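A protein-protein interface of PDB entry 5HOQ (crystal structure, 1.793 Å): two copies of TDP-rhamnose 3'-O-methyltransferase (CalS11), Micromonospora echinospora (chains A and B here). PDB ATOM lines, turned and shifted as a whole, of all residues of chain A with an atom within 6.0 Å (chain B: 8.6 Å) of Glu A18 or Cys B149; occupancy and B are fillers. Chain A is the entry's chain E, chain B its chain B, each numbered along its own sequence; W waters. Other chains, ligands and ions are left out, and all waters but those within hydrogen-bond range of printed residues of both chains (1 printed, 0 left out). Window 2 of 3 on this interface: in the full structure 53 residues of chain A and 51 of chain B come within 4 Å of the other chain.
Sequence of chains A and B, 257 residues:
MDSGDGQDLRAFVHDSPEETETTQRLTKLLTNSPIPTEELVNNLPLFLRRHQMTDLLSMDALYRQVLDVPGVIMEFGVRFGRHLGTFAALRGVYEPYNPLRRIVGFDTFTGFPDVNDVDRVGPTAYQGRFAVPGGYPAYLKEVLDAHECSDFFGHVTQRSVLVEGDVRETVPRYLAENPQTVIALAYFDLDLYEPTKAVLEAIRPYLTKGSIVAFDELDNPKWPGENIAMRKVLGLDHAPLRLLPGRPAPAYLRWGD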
ATOM      1  N   SER A  16     -23.011 -14.659  15.016  1.00  0.00           N
ATOM      2  CA  SER A  16     -24.110 -15.299  15.729  1.00  0.00           C
ATOM      3  C   SER A  16     -23.875 -16.809  15.842  1.00  0.00           C
ATOM      4  O   SER A  16     -23.060 -17.382  15.114  1.00  0.00           O
ATOM      5  CB  SER A  16     -25.428 -15.046  15.000  1.00  0.00           C
ATOM      6  OG  SER A  16     -25.493 -15.847  13.833  1.00  0.00           O
ATOM      7  N   PRO A  17     -24.588 -17.480  16.747  1.00  0.00           N
ATOM      8  CA  PRO A  17     -24.511 -18.958  16.784  1.00  0.00           C
ATOM      9  C   PRO A  17     -24.978 -19.613  15.492  1.00  0.00           C
ATOM     10  O   PRO A  17     -24.418 -20.632  15.065  1.00  0.00           O
ATOM     11  CB  PRO A  17     -25.428 -19.324  17.957  1.00  0.00           C
ATOM     12  CG  PRO A  17     -25.513 -18.080  18.795  1.00  0.00           C
ATOM     13  CD  PRO A  17     -25.424 -16.934  17.830  1.00  0.00           C
ATOM     14  N   GLU A  18     -26.003 -19.037  14.856  1.00  0.00           N
ATOM     15  CA  GLU A  18     -26.530 -19.576  13.599  1.00  0.00           C
ATOM     16  C   GLU A  18     -25.526 -19.425  12.463  1.00  0.00           C
ATOM     17  O   GLU A  18     -25.428 -20.301  11.595  1.00  0.00           O
ATOM     18  CB  GLU A  18     -27.847 -18.872  13.242  1.00  0.00           C
ATOM     19  CG  GLU A  18     -28.998 -19.111  14.245  1.00  0.00           C
ATOM     20  CD  GLU A  18     -28.864 -18.329  15.559  1.00  0.00           C
ATOM     21  OE1 GLU A  18     -28.056 -17.373  15.636  1.00  0.00           O
ATOM     22  OE2 GLU A  18     -29.571 -18.678  16.529  1.00  0.00           O
ATOM     23  N   GLU A  19     -24.790 -18.305  12.435  1.00  0.00           N
ATOM     24  CA  GLU A  19     -23.751 -18.105  11.425  1.00  0.00           C
ATOM     25  C   GLU A  19     -22.630 -19.111  11.619  1.00  0.00           C
ATOM     26  O   GLU A  19     -22.136 -19.711  10.658  1.00  0.00           O
ATOM     27  CB  GLU A  19     -23.216 -16.674  11.516  1.00  0.00           C
ATOM     28  CG  GLU A  19     -21.853 -16.408  10.831  1.00  0.00           C
ATOM     29  CD  GLU A  19     -21.935 -16.207   9.310  1.00  0.00           C
ATOM     30  OE1 GLU A  19     -23.042 -16.318   8.731  1.00  0.00           O
ATOM     31  OE2 GLU A  19     -20.878 -15.922   8.694  1.00  0.00           O
ATOM     32  N   THR A  20     -22.225 -19.310  12.863  1.00  0.00           N
ATOM     33  CA  THR A  20     -21.267 -20.362  13.163  1.00  0.00           C
ATOM     34  C   THR A  20     -21.806 -21.730  12.756  1.00  0.00           C
ATOM     35  O   THR A  20     -21.085 -22.533  12.156  1.00  0.00           O
ATOM     36  CB  THR A  20     -20.921 -20.316  14.650  1.00  0.00           C
ATOM     37  OG1 THR A  20     -20.304 -19.053  14.946  1.00  0.00           O
ATOM     38  CG2 THR A  20     -19.956 -21.448  15.033  1.00  0.00           C
ATOM     39  N   GLU A  21     -23.073 -22.016  13.077  1.00  0.00           N
ATOM     40  CA  GLU A  21     -23.655 -23.301  12.705  1.00  0.00           C
ATOM     41  C   GLU A  21     -23.594 -23.503  11.197  1.00  0.00           C
ATOM     42  O   GLU A  21     -23.171 -24.562  10.724  1.00  0.00           O
ATOM     43  CB  GLU A  21     -25.098 -23.396  13.206  1.00  0.00           C
ATOM     44  CG  GLU A  21     -25.819 -24.718  12.914  1.00  0.00           C
ATOM     45  CD  GLU A  21     -25.101 -25.954  13.493  1.00  0.00           C
ATOM     46  OE1 GLU A  21     -24.241 -25.802  14.394  1.00  0.00           O
ATOM     47  OE2 GLU A  21     -25.397 -27.083  13.038  1.00  0.00           O
ATOM     48  N   THR A  22     -24.006 -22.488  10.420  1.00  0.00           N
ATOM     49  CA  THR A  22     -23.936 -22.599   8.965  1.00  0.00           C
ATOM     50  C   THR A  22     -22.519 -22.875   8.494  1.00  0.00           C
ATOM     51  O   THR A  22     -22.295 -23.702   7.604  1.00  0.00           O
ATOM     52  CB  THR A  22     -24.439 -21.314   8.290  1.00  0.00           C
ATOM     53  OG1 THR A  22     -25.859 -21.254   8.398  1.00  0.00           O
ATOM     54  CG2 THR A  22     -24.060 -21.288   6.813  1.00  0.00           C
ATOM     55  N   THR A  23     -21.556 -22.131   9.027  1.00  0.00           N
ATOM     56  CA  THR A  23     -20.172 -22.267   8.584  1.00  0.00           C
ATOM     57  C   THR A  23     -19.646 -23.664   8.872  1.00  0.00           C
ATOM     58  O   THR A  23     -19.012 -24.286   8.015  1.00  0.00           O
ATOM     59  CB  THR A  23     -19.312 -21.192   9.274  1.00  0.00           C
ATOM     60  OG1 THR A  23     -19.804 -19.889   8.917  1.00  0.00           O
ATOM     61  CG2 THR A  23     -17.830 -21.292   8.892  1.00  0.00           C
ATOM     62  N   ARG A  25     -21.446 -26.467   9.336  1.00  0.00           N
ATOM     63  CA  ARG A  25     -22.157 -27.479   8.556  1.00  0.00           C
ATOM     64  C   ARG A  25     -21.632 -27.538   7.140  1.00  0.00           C
ATOM     65  O   ARG A  25     -21.400 -28.624   6.597  1.00  0.00           O
ATOM     66  CB  ARG A  25     -23.656 -27.190   8.510  1.00  0.00           C
ATOM     67  CG  ARG A  25     -24.387 -27.401   9.791  1.00  0.00           C
ATOM     68  CD  ARG A  25     -25.878 -27.522   9.500  1.00  0.00           C
ATOM     69  NE  ARG A  25     -26.684 -27.234  10.665  1.00  0.00           N
ATOM     70  CZ  ARG A  25     -28.011 -27.322  10.685  1.00  0.00           C
ATOM     71  NH1 ARG A  25     -28.674 -27.699   9.594  1.00  0.00           N
ATOM     72  NH2 ARG A  25     -28.670 -27.033  11.797  1.00  0.00           N
ATOM     73  N   ARG B  91     -30.528 -15.129  -2.068  1.00  0.00           N
ATOM     74  CA  ARG B  91     -31.751 -14.833  -1.332  1.00  0.00           C
ATOM     75  C   ARG B  91     -31.437 -14.236   0.028  1.00  0.00           C
ATOM     76  O   ARG B  91     -32.172 -13.364   0.512  1.00  0.00           O
ATOM     77  CB  ARG B  91     -32.602 -16.092  -1.180  1.00  0.00           C
ATOM     78  CG  ARG B  91     -33.932 -15.878  -0.511  1.00  0.00           C
ATOM     79  CD  ARG B  91     -34.757 -17.165  -0.536  1.00  0.00           C
ATOM     80  NE  ARG B  91     -34.064 -18.272   0.162  1.00  0.00           N
ATOM     81  CZ  ARG B  91     -34.477 -19.537   0.199  1.00  0.00           C
ATOM     82  NH1 ARG B  91     -35.591 -19.902  -0.414  1.00  0.00           N
ATOM     83  NH2 ARG B  91     -33.773 -20.451   0.864  1.00  0.00           N
ATOM     84  N   GLU B 142     -29.465 -31.213   2.639  1.00  0.00           N
ATOM     85  CA  GLU B 142     -28.675 -30.855   3.812  1.00  0.00           C
ATOM     86  C   GLU B 142     -27.834 -29.612   3.552  1.00  0.00           C
ATOM     87  O   GLU B 142     -27.652 -28.774   4.448  1.00  0.00           O
ATOM     88  CB  GLU B 142     -27.778 -32.035   4.212  1.00  0.00           C
ATOM     89  CG  GLU B 142     -27.789 -32.340   5.678  1.00  0.00           C
ATOM     90  CD  GLU B 142     -26.884 -33.505   6.037  1.00  0.00           C
ATOM     91  OE1 GLU B 142     -26.932 -34.544   5.343  1.00  0.00           O
ATOM     92  OE2 GLU B 142     -26.123 -33.369   7.013  1.00  0.00           O
ATOM     93  N   VAL B 143     -27.303 -29.477   2.337  1.00  0.00           N
ATOM     94  CA  VAL B 143     -26.549 -28.274   1.992  1.00  0.00           C
ATOM     95  C   VAL B 143     -27.461 -27.050   2.047  1.00  0.00           C
ATOM     96  O   VAL B 143     -27.116 -26.006   2.626  1.00  0.00           O
ATOM     97  CB  VAL B 143     -25.896 -28.444   0.610  1.00  0.00           C
ATOM     98  CG1 VAL B 143     -25.312 -27.134   0.131  1.00  0.00           C
ATOM     99  CG2 VAL B 143     -24.805 -29.521   0.664  1.00  0.00           C
ATOM    100  N   LEU B 144     -28.643 -27.155   1.444  1.00  0.00           N
ATOM    101  CA  LEU B 144     -29.548 -26.006   1.426  1.00  0.00           C
ATOM    102  C   LEU B 144     -30.059 -25.682   2.830  1.00  0.00           C
ATOM    103  O   LEU B 144     -30.135 -24.504   3.216  1.00  0.00           O
ATOM    104  CB  LEU B 144     -30.695 -26.272   0.457  1.00  0.00           C
ATOM    105  CG  LEU B 144     -30.273 -26.399  -1.014  1.00  0.00           C
ATOM    106  CD1 LEU B 144     -31.428 -26.928  -1.864  1.00  0.00           C
ATOM    107  CD2 LEU B 144     -29.730 -25.082  -1.585  1.00  0.00           C
ATOM    108  N   ASP B 145     -30.366 -26.708   3.630  1.00  0.00           N
ATOM    109  CA  ASP B 145     -30.727 -26.476   5.024  1.00  0.00           C
ATOM    110  C   ASP B 145     -29.619 -25.751   5.789  1.00  0.00           C
ATOM    111  O   ASP B 145     -29.909 -24.984   6.712  1.00  0.00           O
ATOM    112  CB  ASP B 145     -31.031 -27.796   5.727  1.00  0.00           C
ATOM    113  CG  ASP B 145     -32.346 -28.423   5.272  1.00  0.00           C
ATOM    114  OD1 ASP B 145     -33.168 -27.750   4.612  1.00  0.00           O
ATOM    115  OD2 ASP B 145     -32.549 -29.607   5.593  1.00  0.00           O
ATOM    116  N   ALA B 146     -28.354 -26.017   5.469  1.00  0.00           N
ATOM    117  CA  ALA B 146     -27.272 -25.356   6.201  1.00  0.00           C
ATOM    118  C   ALA B 146     -27.225 -23.869   5.897  1.00  0.00           C
ATOM    119  O   ALA B 146     -26.925 -23.063   6.784  1.00  0.00           O
ATOM    120  CB  ALA B 146     -25.921 -26.001   5.893  1.00  0.00           C
ATOM    121  N   HIS B 147     -27.507 -23.479   4.650  1.00  0.00           N
ATOM    122  CA  HIS B 147     -27.678 -22.061   4.344  1.00  0.00           C
ATOM    123  C   HIS B 147     -28.858 -21.499   5.112  1.00  0.00           C
ATOM    124  O   HIS B 147     -28.773 -20.426   5.717  1.00  0.00           O
ATOM    125  CB  HIS B 147     -27.903 -21.848   2.852  1.00  0.00           C
ATOM    126  CG  HIS B 147     -26.693 -22.057   2.004  1.00  0.00           C
ATOM    127  ND1 HIS B 147     -25.880 -21.018   1.601  1.00  0.00           N
ATOM    128  CD2 HIS B 147     -26.186 -23.177   1.432  1.00  0.00           C
ATOM    129  CE1 HIS B 147     -24.902 -21.494   0.850  1.00  0.00           C
ATOM    130  NE2 HIS B 147     -25.071 -22.801   0.719  1.00  0.00           N
ATOM    131  N   GLU B 148     -29.975 -22.228   5.104  1.00  0.00           N
ATOM    132  CA  GLU B 148     -31.212 -21.698   5.644  1.00  0.00           C
ATOM    133  C   GLU B 148     -31.189 -21.558   7.162  1.00  0.00           C
ATOM    134  O   GLU B 148     -31.912 -20.719   7.700  1.00  0.00           O
ATOM    135  CB  GLU B 148     -32.377 -22.586   5.187  1.00  0.00           C
ATOM    136  CG  GLU B 148     -32.658 -22.402   3.712  1.00  0.00           C
ATOM    137  CD  GLU B 148     -33.854 -23.195   3.241  1.00  0.00           C
ATOM    138  OE1 GLU B 148     -34.348 -24.034   4.022  1.00  0.00           O
ATOM    139  OE2 GLU B 148     -34.311 -22.972   2.093  1.00  0.00           O
ATOM    140  N   CYS B 149     -30.363 -22.319   7.881  1.00  0.00           N
ATOM    141  CA  CYS B 149     -30.492 -22.185   9.326  1.00  0.00           C
ATOM    142  C   CYS B 149     -29.974 -20.851   9.851  1.00  0.00           C
ATOM    143  O   CYS B 149     -30.242 -20.535  11.015  1.00  0.00           O
ATOM    144  CB  CYS B 149     -29.818 -23.353  10.042  1.00  0.00           C
ATOM    145  SG  CYS B 149     -28.075 -23.355   9.969  1.00  0.00           S
ATOM    146  N   SER B 150     -29.294 -20.035   9.037  1.00  0.00           N
ATOM    147  CA  SER B 150     -28.913 -18.699   9.472  1.00  0.00           C
ATOM    148  C   SER B 150     -29.703 -17.597   8.755  1.00  0.00           C
ATOM    149  O   SER B 150     -29.393 -16.416   8.930  1.00  0.00           O
ATOM    150  CB  SER B 150     -27.396 -18.489   9.313  1.00  0.00           C
ATOM    151  OG  SER B 150     -26.960 -18.656   7.980  1.00  0.00           O
ATOM    152  N   ASP B 151     -30.725 -17.950   7.975  1.00  0.00           N
ATOM    153  CA  ASP B 151     -31.628 -16.953   7.407  1.00  0.00           C
ATOM    154  C   ASP B 151     -32.510 -16.324   8.481  1.00  0.00           C
ATOM    155  O   ASP B 151     -32.912 -16.966   9.464  1.00  0.00           O
ATOM    156  CB  ASP B 151     -32.557 -17.571   6.354  1.00  0.00           C
ATOM    157  CG  ASP B 151     -31.866 -17.883   5.036  1.00  0.00           C
ATOM    158  OD1 ASP B 151     -30.872 -17.220   4.690  1.00  0.00           O
ATOM    159  OD2 ASP B 151     -32.364 -18.785   4.331  1.00  0.00           O
ATOM    160  N   PHE B 152     -32.877 -15.071   8.237  1.00  0.00           N
ATOM    161  CA  PHE B 152     -33.792 -14.370   9.130  1.00  0.00           C
ATOM    162  C   PHE B 152     -35.114 -15.125   9.287  1.00  0.00           C
ATOM    163  O   PHE B 152     -35.686 -15.160  10.382  1.00  0.00           O
ATOM    164  CB  PHE B 152     -34.027 -12.958   8.611  1.00  0.00           C
ATOM    165  CG  PHE B 152     -34.773 -12.097   9.567  1.00  0.00           C
ATOM    166  CD1 PHE B 152     -36.153 -12.039   9.534  1.00  0.00           C
ATOM    167  CD2 PHE B 152     -34.090 -11.374  10.530  1.00  0.00           C
ATOM    168  CE1 PHE B 152     -36.851 -11.223  10.435  1.00  0.00           C
ATOM    169  CE2 PHE B 152     -34.769 -10.576  11.437  1.00  0.00           C
ATOM    170  CZ  PHE B 152     -36.154 -10.513  11.398  1.00  0.00           C
ATOM    171  N   PHE B 153     -35.611 -15.756   8.216  1.00  0.00           N
ATOM    172  CA  PHE B 153     -36.806 -16.586   8.311  1.00  0.00           C
ATOM    173  C   PHE B 153     -36.489 -18.080   8.321  1.00  0.00           C
ATOM    174  O   PHE B 153     -37.280 -18.894   7.843  1.00  0.00           O
ATOM    175  CB  PHE B 153     -37.781 -16.257   7.183  1.00  0.00           C
ATOM    176  CG  PHE B 153     -38.744 -15.168   7.542  1.00  0.00           C
ATOM    177  CD1 PHE B 153     -39.842 -15.432   8.369  1.00  0.00           C
ATOM    178  CD2 PHE B 153     -38.553 -13.874   7.089  1.00  0.00           C
ATOM    179  CE1 PHE B 153     -40.725 -14.414   8.728  1.00  0.00           C
ATOM    180  CE2 PHE B 153     -39.439 -12.849   7.439  1.00  0.00           C
ATOM    181  CZ  PHE B 153     -40.522 -13.120   8.261  1.00  0.00           C
ATOM    182  N   GLY B 154     -35.355 -18.463   8.889  1.00  0.00           N
ATOM    183  CA  GLY B 154     -34.973 -19.857   8.901  1.00  0.00           C
ATOM    184  C   GLY B 154     -35.914 -20.765   9.674  1.00  0.00           C
ATOM    185  O   GLY B 154     -35.818 -21.988   9.527  1.00  0.00           O
ATOM    186  N   HIS B 155     -36.803 -20.215  10.494  1.00  0.00           N
ATOM    187  CA  HIS B 155     -37.802 -21.043  11.168  1.00  0.00           C
ATOM    188  C   HIS B 155     -38.963 -21.458  10.267  1.00  0.00           C
ATOM    189  O   HIS B 155     -39.751 -22.319  10.673  1.00  0.00           O
ATOM    190  CB  HIS B 155     -38.354 -20.301  12.387  1.00  0.00           C
ATOM    191  CG  HIS B 155     -38.982 -18.980  12.052  1.00  0.00           C
ATOM    192  ND1 HIS B 155     -38.246 -17.886  11.652  1.00  0.00           N
ATOM    193  CD2 HIS B 155     -40.276 -18.584  12.048  1.00  0.00           C
ATOM    194  CE1 HIS B 155     -39.065 -16.870  11.426  1.00  0.00           C
ATOM    195  NE2 HIS B 155     -40.302 -17.271  11.650  1.00  0.00           N
ATOM    196  N   VAL B 156     -39.121 -20.865   9.082  1.00  0.00           N
ATOM    197  CA  VAL B 156     -40.158 -21.284   8.138  1.00  0.00           C
ATOM    198  C   VAL B 156     -39.604 -22.393   7.251  1.00  0.00           C
ATOM    199  O   VAL B 156     -38.556 -22.227   6.613  1.00  0.00           O
ATOM    200  CB  VAL B 156     -40.643 -20.096   7.288  1.00  0.00           C
ATOM    201  CG1 VAL B 156     -41.677 -20.545   6.294  1.00  0.00           C
ATOM    202  CG2 VAL B 156     -41.232 -18.997   8.170  1.00  0.00           C
ATOM    203  N   ARG B 159     -38.761 -23.737   2.318  1.00  0.00           N
ATOM    204  CA  ARG B 159     -38.305 -22.639   1.485  1.00  0.00           C
ATOM    205  C   ARG B 159     -37.321 -23.102   0.425  1.00  0.00           C
ATOM    206  O   ARG B 159     -36.999 -22.332  -0.484  1.00  0.00           O
ATOM    207  CB  ARG B 159     -37.689 -21.535   2.365  1.00  0.00           C
ATOM    208  CG  ARG B 159     -38.759 -20.803   3.165  1.00  0.00           C
ATOM    209  CD  ARG B 159     -38.205 -19.604   3.934  1.00  0.00           C
ATOM    210  NE  ARG B 159     -37.064 -19.999   4.738  1.00  0.00           N
ATOM    211  CZ  ARG B 159     -35.816 -19.563   4.570  1.00  0.00           C
ATOM    212  NH1 ARG B 159     -35.519 -18.665   3.653  1.00  0.00           N
ATOM    213  NH2 ARG B 159     -34.862 -20.032   5.365  1.00  0.00           N
HETATM  214  O   HOH W   1     -27.686 -29.141   7.109  1.00  0.00           O
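OG1 of Thr A22 is in hydrogen-bond range of SG of Cys B149 (3.4 Å).
O of Ala B146 lies within hydrogen-bond range of OG1 of Thr A22 (2.6 Å).
The side-chain hydroxyl of Ser B150 sits at hydrogen-bond distance from the side-chain hydroxyl of Thr A22 (2.9 Å).
SG of Cys B149 is in hydrogen-bond range of O of Ala B146.
OE2 of Glu A21 lies within salt-bridge range of NE of Arg A25 (2.7 Å).
The side-chain hydroxyl (OG) of Ser A16 lies close to the backbone NH (N) of Glu A18 (3.4 Å).
The side-chain hydroxyl (OG) of Ser B150 lies within hydrogen-bond range of the backbone carbonyl oxygen (O) of His B147.
The backbone carbonyl oxygen of Glu A18 lies within hydrogen-bond range of the side-chain hydroxyl of Thr A22, at 3.4 Å.
Among the printed residues, pairs that only touch across the chains: Glu A18 with Ser B150, Arg A25 with Ala B146, Glu A18 with Cys B149 and Glu A21 with Cys B149.
Glu A18 touches two residues of chain B.
Printed residues of chain B within 4 Å of Glu A21: Cys B149 (3.95 Å).
Printed residues of chain B within 4 Å of Thr A22: Ala B146, Cys B149 and Ser B150.
Of the printed residues of chain B, Arg A25 touches Ala B146 (3.7 Å).
Printed residues of chain A within 4 Å of Ala B146: Thr A22 and Arg A25.
Cys B149 touches three residues of chain A.
Printed residues of chain A within 4 Å of Ser B150: Glu A18 (3.5 Å) and Thr A22 (2.9 Å).
Arg B159 touches none of the printed residues of chain A.
The nearest printed residue of chain B that does not touch Arg A25 is Cys B149 (4.03 Å).
Of the 17 printed residues of chain B, 3 touch a printed residue of chain A.
Of the 9 printed residues of chain A, 4 touch a printed residue of chain B.
Among the printed residues, 7 pairs touch across the chains.
Among the printed residues, no Asp or Glu carboxylate lies within 4 Å of a Lys or Arg side-chain nitrogen of the other chain.
No position is printed for both chains.
Of the 7 pairs that touch across the chains among the printed residues, none has its exchanged pair printed and touching as well.
Water W1 lies within hydrogen-bond range of O of Glu B142 (2.7 Å) and NH1 of Arg A25 (3.0 Å).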
